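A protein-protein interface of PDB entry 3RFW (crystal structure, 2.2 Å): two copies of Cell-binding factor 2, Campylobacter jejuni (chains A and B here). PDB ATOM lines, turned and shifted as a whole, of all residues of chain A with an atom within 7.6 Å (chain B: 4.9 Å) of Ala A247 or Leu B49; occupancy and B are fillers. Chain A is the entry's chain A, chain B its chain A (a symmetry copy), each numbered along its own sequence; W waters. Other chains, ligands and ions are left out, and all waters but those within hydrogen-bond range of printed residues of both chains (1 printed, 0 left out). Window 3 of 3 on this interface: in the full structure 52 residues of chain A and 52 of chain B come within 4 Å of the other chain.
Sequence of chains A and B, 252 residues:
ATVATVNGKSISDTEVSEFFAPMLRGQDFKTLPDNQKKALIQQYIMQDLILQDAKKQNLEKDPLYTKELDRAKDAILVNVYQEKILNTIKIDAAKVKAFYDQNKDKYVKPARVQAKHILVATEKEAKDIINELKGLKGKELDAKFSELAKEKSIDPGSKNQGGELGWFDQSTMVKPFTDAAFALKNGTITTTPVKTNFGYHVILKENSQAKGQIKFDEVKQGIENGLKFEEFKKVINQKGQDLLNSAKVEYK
The backbone carbonyl oxygen (O) of Gly A240 lies close to the side-chain sulfur (SD) of Met B46 (3.4 Å).
O of Lys A248 sits at hydrogen-bond distance from N of Asn B7 (2.7 Å).
OH of Tyr A81 lies within hydrogen-bond range of OD1 of Asp B53 (2.6 Å).
CG2 of Val A78 touches CD2 of Leu B51, at 3.8 Å.
CD1 of Tyr A81 touches CG2 of Ile B50, at 3.5 Å.
Leu A243 touches Leu B49.
Leu A243 touches Ile B50.
CD2 of Leu A243 touches CG of Asp B53 (3.7 Å).
CE of Met B46 touches CD1 of Leu A244, at 3.8 Å.
Leu A244 touches Leu B49 (CD2 to CD1, 3.9 Å).
Asn B7 touches Ala A247.
Ala A247 touches Leu B49.
CA of Val B6 touches O of Lys A248, 3.4 Å away.
Printed residues of chain B within 4 Å of Leu A244: Met B46 and Leu B49.
Ala A247 touches two residues of chain B.
Printed residues of chain B within 4 Å of Lys A248: Val B6 (3.4 Å) and Asn B7 (2.7 Å).
Printed residues of chain A within 4 Å of Val B6: Lys A248.
Leu B49 touches just these residues of chain A: Leu A243, Leu A244 and Ala A247.
Printed residues of chain A within 4 Å of Ile B50: Tyr A81 and Leu A243.
Printed residues of chain A within 4 Å of Asp B53: Tyr A81 and Leu A243.
The nearest residue of chain B that does not touch Ala A247 is Val B6 (4.2 Å).
The nearest residue of chain A that does not touch Leu B49 is Val A249 (5.0 Å).
Of the 11 printed residues of chain B, 7 touch a printed residue of chain A.
Printed residues of chain B that touch a printed residue of chain A: Val B6, Asn B7, Met B46, Leu B49, Ile B50, Leu B51 and Asp B53.
Among the printed residues, no Asp or Glu carboxylate lies within 4 Å of a Lys or Arg side-chain nitrogen of the other chain.
No position is printed for both chains.
Of the 13 pairs that touch across the chains among the printed residues, none has its exchanged pair printed and touching as well.
Water W1 bridges the backbone carbonyl oxygen (O) of Lys A248 (2.7 Å) and the backbone NH (N) of Asn B7 (3.4 Å).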
ATOM      1  N   VAL A  78      -6.143 -10.848 -32.672  1.00  0.00           N
ATOM      2  CA  VAL A  78      -7.575 -10.764 -32.420  1.00  0.00           C
ATOM      3  C   VAL A  78      -8.305 -10.628 -33.751  1.00  0.00           C
ATOM      4  O   VAL A  78      -9.311 -11.276 -33.977  1.00  0.00           O
ATOM      5  CB  VAL A  78      -7.913  -9.599 -31.487  1.00  0.00           C
ATOM      6  CG1 VAL A  78      -9.434  -9.276 -31.519  1.00  0.00           C
ATOM      7  CG2 VAL A  78      -7.483  -9.906 -30.090  1.00  0.00           C
ATOM      8  N   TYR A  81      -8.289 -13.924 -35.641  1.00  0.00           N
ATOM      9  CA  TYR A  81      -9.311 -14.746 -34.992  1.00  0.00           C
ATOM     10  C   TYR A  81     -10.713 -14.414 -35.511  1.00  0.00           C
ATOM     11  O   TYR A  81     -11.438 -15.311 -35.890  1.00  0.00           O
ATOM     12  CB  TYR A  81      -9.246 -14.540 -33.482  1.00  0.00           C
ATOM     13  CG  TYR A  81     -10.092 -15.486 -32.649  1.00  0.00           C
ATOM     14  CD1 TYR A  81     -11.348 -15.100 -32.167  1.00  0.00           C
ATOM     15  CD2 TYR A  81      -9.618 -16.752 -32.304  1.00  0.00           C
ATOM     16  CE1 TYR A  81     -12.112 -15.973 -31.362  1.00  0.00           C
ATOM     17  CE2 TYR A  81     -10.372 -17.621 -31.518  1.00  0.00           C
ATOM     18  CZ  TYR A  81     -11.593 -17.209 -31.013  1.00  0.00           C
ATOM     19  OH  TYR A  81     -12.323 -18.089 -30.248  1.00  0.00           O
ATOM     20  N   GLY A 240     -17.936 -15.140 -27.823  1.00  0.00           N
ATOM     21  CA  GLY A 240     -17.416 -14.338 -26.739  1.00  0.00           C
ATOM     22  C   GLY A 240     -18.019 -14.805 -25.423  1.00  0.00           C
ATOM     23  O   GLY A 240     -17.384 -14.681 -24.363  1.00  0.00           O
ATOM     24  N   GLN A 241     -19.226 -15.368 -25.522  1.00  0.00           N
ATOM     25  CA  GLN A 241     -19.918 -16.056 -24.446  1.00  0.00           C
ATOM     26  C   GLN A 241     -19.355 -17.429 -24.092  1.00  0.00           C
ATOM     27  O   GLN A 241     -19.319 -17.795 -22.925  1.00  0.00           O
ATOM     28  CB  GLN A 241     -21.406 -16.231 -24.815  1.00  0.00           C
ATOM     29  N   ASP A 242     -19.036 -18.245 -25.090  1.00  0.00           N
ATOM     30  CA  ASP A 242     -18.481 -19.536 -24.788  1.00  0.00           C
ATOM     31  C   ASP A 242     -17.176 -19.389 -23.999  1.00  0.00           C
ATOM     32  O   ASP A 242     -16.846 -20.268 -23.203  1.00  0.00           O
ATOM     33  CB  ASP A 242     -18.267 -20.396 -26.047  1.00  0.00           C
ATOM     34  CG  ASP A 242     -19.581 -20.772 -26.753  1.00  0.00           C
ATOM     35  OD1 ASP A 242     -20.671 -20.579 -26.150  1.00  0.00           O
ATOM     36  OD2 ASP A 242     -19.519 -21.207 -27.933  1.00  0.00           O
ATOM     37  N   LEU A 243     -16.435 -18.294 -24.225  1.00  0.00           N
ATOM     38  CA  LEU A 243     -15.045 -18.206 -23.774  1.00  0.00           C
ATOM     39  C   LEU A 243     -15.090 -17.722 -22.347  1.00  0.00           C
ATOM     40  O   LEU A 243     -14.357 -18.196 -21.476  1.00  0.00           O
ATOM     41  CB  LEU A 243     -14.219 -17.220 -24.631  1.00  0.00           C
ATOM     42  CG  LEU A 243     -13.855 -17.613 -26.065  1.00  0.00           C
ATOM     43  CD1 LEU A 243     -13.094 -16.469 -26.756  1.00  0.00           C
ATOM     44  CD2 LEU A 243     -13.043 -18.922 -26.096  1.00  0.00           C
ATOM     45  N   LEU A 244     -15.946 -16.743 -22.135  1.00  0.00           N
ATOM     46  CA  LEU A 244     -16.131 -16.150 -20.818  1.00  0.00           C
ATOM     47  C   LEU A 244     -16.691 -17.141 -19.783  1.00  0.00           C
ATOM     48  O   LEU A 244     -16.251 -17.161 -18.631  1.00  0.00           O
ATOM     49  CB  LEU A 244     -17.063 -14.947 -20.922  1.00  0.00           C
ATOM     50  CG  LEU A 244     -16.452 -13.584 -20.633  1.00  0.00           C
ATOM     51  CD1 LEU A 244     -17.575 -12.548 -20.486  1.00  0.00           C
ATOM     52  CD2 LEU A 244     -15.657 -13.680 -19.337  1.00  0.00           C
ATOM     53  N   ASN A 245     -17.668 -17.934 -20.202  1.00  0.00           N
ATOM     54  CA  ASN A 245     -18.381 -18.824 -19.296  1.00  0.00           C
ATOM     55  C   ASN A 245     -17.364 -19.830 -18.752  1.00  0.00           C
ATOM     56  O   ASN A 245     -17.231 -19.983 -17.520  1.00  0.00           O
ATOM     57  CB  ASN A 245     -19.456 -19.631 -20.054  1.00  0.00           C
ATOM     58  CG  ASN A 245     -20.737 -18.835 -20.332  1.00  0.00           C
ATOM     59  OD1 ASN A 245     -20.867 -17.644 -19.978  1.00  0.00           O
ATOM     60  ND2 ASN A 245     -21.663 -19.480 -21.048  1.00  0.00           N
ATOM     61  N   SER A 246     -16.862 -20.611 -19.723  1.00  0.00           N
ATOM     62  CA  SER A 246     -15.633 -21.414 -19.742  1.00  0.00           C
ATOM     63  C   SER A 246     -14.492 -21.035 -18.813  1.00  0.00           C
ATOM     64  O   SER A 246     -13.814 -21.912 -18.298  1.00  0.00           O
ATOM     65  CB  SER A 246     -15.099 -21.465 -21.160  1.00  0.00           C
ATOM     66  OG  SER A 246     -14.802 -22.773 -21.599  1.00  0.00           O
ATOM     67  N   ALA A 247     -14.270 -19.745 -18.621  1.00  0.00           N
ATOM     68  CA  ALA A 247     -13.188 -19.264 -17.766  1.00  0.00           C
ATOM     69  C   ALA A 247     -13.723 -19.062 -16.366  1.00  0.00           C
ATOM     70  O   ALA A 247     -14.863 -18.697 -16.212  1.00  0.00           O
ATOM     71  CB  ALA A 247     -12.626 -17.913 -18.288  1.00  0.00           C
ATOM     72  N   LYS A 248     -12.839 -19.157 -15.384  1.00  0.00           N
ATOM     73  CA  LYS A 248     -13.120 -18.757 -14.028  1.00  0.00           C
ATOM     74  C   LYS A 248     -12.593 -17.354 -13.744  1.00  0.00           C
ATOM     75  O   LYS A 248     -11.370 -17.133 -13.629  1.00  0.00           O
ATOM     76  CB  LYS A 248     -12.481 -19.750 -13.048  1.00  0.00           C
ATOM     77  N   VAL A 249     -13.535 -16.438 -13.540  1.00  0.00           N
ATOM     78  CA  VAL A 249     -13.295 -15.010 -13.485  1.00  0.00           C
ATOM     79  C   VAL A 249     -13.709 -14.419 -12.135  1.00  0.00           C
ATOM     80  O   VAL A 249     -14.859 -14.510 -11.752  1.00  0.00           O
ATOM     81  CB  VAL A 249     -14.077 -14.309 -14.618  1.00  0.00           C
ATOM     82  CG1 VAL A 249     -14.001 -12.779 -14.464  1.00  0.00           C
ATOM     83  CG2 VAL A 249     -13.542 -14.753 -15.993  1.00  0.00           C
ATOM     84  N   GLU A 250     -12.782 -13.789 -11.427  1.00  0.00           N
ATOM     85  CA  GLU A 250     -13.111 -13.091 -10.193  1.00  0.00           C
ATOM     86  C   GLU A 250     -12.780 -11.594 -10.282  1.00  0.00           C
ATOM     87  O   GLU A 250     -11.643 -11.225 -10.557  1.00  0.00           O
ATOM     88  CB  GLU A 250     -12.369 -13.731  -9.003  1.00  0.00           C
ATOM     89  CG  GLU A 250     -12.157 -15.261  -9.110  1.00  0.00           C
ATOM     90  CD  GLU A 250     -13.370 -16.063  -8.671  1.00  0.00           C
ATOM     91  OE1 GLU A 250     -14.124 -15.540  -7.839  1.00  0.00           O
ATOM     92  N   VAL B   6      -8.221 -14.374 -13.805  1.00  0.00           N
ATOM     93  CA  VAL B   6      -8.844 -15.164 -14.844  1.00  0.00           C
ATOM     94  C   VAL B   6      -8.138 -16.487 -14.862  1.00  0.00           C
ATOM     95  O   VAL B   6      -6.935 -16.535 -15.117  1.00  0.00           O
ATOM     96  CB  VAL B   6      -8.648 -14.533 -16.229  1.00  0.00           C
ATOM     97  CG1 VAL B   6      -9.335 -15.415 -17.304  1.00  0.00           C
ATOM     98  CG2 VAL B   6      -9.248 -13.124 -16.270  1.00  0.00           C
ATOM     99  N   ASN B   7      -8.884 -17.558 -14.578  1.00  0.00           N
ATOM    100  CA  ASN B   7      -8.327 -18.884 -14.318  1.00  0.00           C
ATOM    101  C   ASN B   7      -7.140 -18.866 -13.357  1.00  0.00           C
ATOM    102  O   ASN B   7      -6.192 -19.614 -13.526  1.00  0.00           O
ATOM    103  CB  ASN B   7      -7.958 -19.586 -15.620  1.00  0.00           C
ATOM    104  CG  ASN B   7      -9.163 -19.839 -16.515  1.00  0.00           C
ATOM    105  OD1 ASN B   7      -9.065 -19.843 -17.753  1.00  0.00           O
ATOM    106  ND2 ASN B   7     -10.286 -20.119 -15.898  1.00  0.00           N
ATOM    107  N   ILE B  45     -10.787  -8.475 -20.420  1.00  0.00           N
ATOM    108  CA  ILE B  45     -10.756  -9.928 -20.134  1.00  0.00           C
ATOM    109  C   ILE B  45     -11.232 -10.736 -21.344  1.00  0.00           C
ATOM    110  O   ILE B  45     -10.675 -11.772 -21.714  1.00  0.00           O
ATOM    111  CB  ILE B  45     -11.642 -10.233 -18.860  1.00  0.00           C
ATOM    112  CG1 ILE B  45     -10.908  -9.718 -17.606  1.00  0.00           C
ATOM    113  CG2 ILE B  45     -11.945 -11.719 -18.782  1.00  0.00           C
ATOM    114  CD1 ILE B  45     -11.760  -9.572 -16.355  1.00  0.00           C
ATOM    115  N   MET B  46     -12.240 -10.219 -22.020  1.00  0.00           N
ATOM    116  CA  MET B  46     -12.756 -10.877 -23.223  1.00  0.00           C
ATOM    117  C   MET B  46     -11.700 -10.869 -24.331  1.00  0.00           C
ATOM    118  O   MET B  46     -11.452 -11.907 -24.976  1.00  0.00           O
ATOM    119  CB  MET B  46     -14.058 -10.198 -23.682  1.00  0.00           C
ATOM    120  CG  MET B  46     -14.512 -10.557 -25.111  1.00  0.00           C
ATOM    121  SD  MET B  46     -15.220 -12.213 -25.060  1.00  0.00           S
ATOM    122  CE  MET B  46     -16.696 -11.804 -24.105  1.00  0.00           C
ATOM    123  N   GLN B  47     -11.078  -9.710 -24.547  1.00  0.00           N
ATOM    124  CA  GLN B  47      -9.885  -9.594 -25.427  1.00  0.00           C
ATOM    125  C   GLN B  47      -8.789 -10.581 -25.002  1.00  0.00           C
ATOM    126  O   GLN B  47      -8.322 -11.350 -25.788  1.00  0.00           O
ATOM    127  CB  GLN B  47      -9.361  -8.128 -25.428  1.00  0.00           C
ATOM    128  CG  GLN B  47      -8.082  -7.846 -26.271  1.00  0.00           C
ATOM    129  CD  GLN B  47      -6.761  -7.958 -25.471  1.00  0.00           C
ATOM    130  OE1 GLN B  47      -6.745  -8.107 -24.236  1.00  0.00           O
ATOM    131  NE2 GLN B  47      -5.650  -7.846 -26.176  1.00  0.00           N
ATOM    132  N   ASP B  48      -8.580 -10.729 -23.712  1.00  0.00           N
ATOM    133  CA  ASP B  48      -7.536 -11.631 -23.248  1.00  0.00           C
ATOM    134  C   ASP B  48      -7.813 -13.091 -23.536  1.00  0.00           C
ATOM    135  O   ASP B  48      -6.923 -13.868 -23.924  1.00  0.00           O
ATOM    136  CB  ASP B  48      -7.281 -11.417 -21.779  1.00  0.00           C
ATOM    137  CG  ASP B  48      -6.050 -12.160 -21.297  1.00  0.00           C
ATOM    138  OD1 ASP B  48      -4.928 -11.689 -21.571  1.00  0.00           O
ATOM    139  OD2 ASP B  48      -6.210 -13.229 -20.662  1.00  0.00           O
ATOM    140  N   LEU B  49      -9.093 -13.431 -23.498  1.00  0.00           N
ATOM    141  CA  LEU B  49      -9.501 -14.808 -23.659  1.00  0.00           C
ATOM    142  C   LEU B  49      -9.537 -15.119 -25.125  1.00  0.00           C
ATOM    143  O   LEU B  49      -9.327 -16.242 -25.506  1.00  0.00           O
ATOM    144  CB  LEU B  49     -10.894 -15.056 -23.028  1.00  0.00           C
ATOM    145  CG  LEU B  49     -10.870 -15.063 -21.483  1.00  0.00           C
ATOM    146  CD1 LEU B  49     -12.294 -15.021 -20.860  1.00  0.00           C
ATOM    147  CD2 LEU B  49     -10.099 -16.274 -20.952  1.00  0.00           C
ATOM    148  N   ILE B  50      -9.831 -14.133 -25.957  1.00  0.00           N
ATOM    149  CA  ILE B  50      -9.789 -14.377 -27.395  1.00  0.00           C
ATOM    150  C   ILE B  50      -8.308 -14.629 -27.807  1.00  0.00           C
ATOM    151  O   ILE B  50      -8.013 -15.514 -28.605  1.00  0.00           O
ATOM    152  CB  ILE B  50     -10.345 -13.194 -28.163  1.00  0.00           C
ATOM    153  CG1 ILE B  50     -11.874 -13.172 -28.083  1.00  0.00           C
ATOM    154  CG2 ILE B  50      -9.837 -13.246 -29.597  1.00  0.00           C
ATOM    155  CD1 ILE B  50     -12.504 -11.845 -28.367  1.00  0.00           C
ATOM    156  N   LEU B  51      -7.383 -13.895 -27.200  1.00  0.00           N
ATOM    157  CA  LEU B  51      -5.929 -14.124 -27.460  1.00  0.00           C
ATOM    158  C   LEU B  51      -5.503 -15.546 -27.082  1.00  0.00           C
ATOM    159  O   LEU B  51      -4.851 -16.227 -27.859  1.00  0.00           O
ATOM    160  CB  LEU B  51      -5.070 -13.115 -26.667  1.00  0.00           C
ATOM    161  CG  LEU B  51      -5.028 -11.651 -27.154  1.00  0.00           C
ATOM    162  CD1 LEU B  51      -4.271 -10.776 -26.165  1.00  0.00           C
ATOM    163  CD2 LEU B  51      -4.424 -11.480 -28.587  1.00  0.00           C
ATOM    164  N   GLN B  52      -5.903 -15.994 -25.889  1.00  0.00           N
ATOM    165  CA  GLN B  52      -5.627 -17.363 -25.446  1.00  0.00           C
ATOM    166  C   GLN B  52      -6.248 -18.395 -26.353  1.00  0.00           C
ATOM    167  O   GLN B  52      -5.635 -19.404 -26.681  1.00  0.00           O
ATOM    168  CB  GLN B  52      -6.122 -17.569 -24.015  1.00  0.00           C
ATOM    169  CG  GLN B  52      -5.456 -16.651 -22.988  1.00  0.00           C
ATOM    170  CD  GLN B  52      -5.842 -17.023 -21.560  1.00  0.00           C
ATOM    171  OE1 GLN B  52      -6.133 -16.159 -20.702  1.00  0.00           O
ATOM    172  NE2 GLN B  52      -5.827 -18.312 -21.294  1.00  0.00           N
ATOM    173  N   ASP B  53      -7.468 -18.141 -26.807  1.00  0.00           N
ATOM    174  CA  ASP B  53      -8.066 -19.079 -27.723  1.00  0.00           C
ATOM    175  C   ASP B  53      -7.379 -19.118 -29.103  1.00  0.00           C
ATOM    176  O   ASP B  53      -7.209 -20.204 -29.698  1.00  0.00           O
ATOM    177  CB  ASP B  53      -9.566 -18.872 -27.843  1.00  0.00           C
ATOM    178  CG  ASP B  53     -10.280 -20.133 -28.284  1.00  0.00           C
ATOM    179  OD1 ASP B  53     -11.049 -20.083 -29.256  1.00  0.00           O
ATOM    180  OD2 ASP B  53      -9.957 -21.202 -27.740  1.00  0.00           O
HETATM  181  O   HOH W   1      -9.834 -16.581 -11.508  1.00  0.00           O
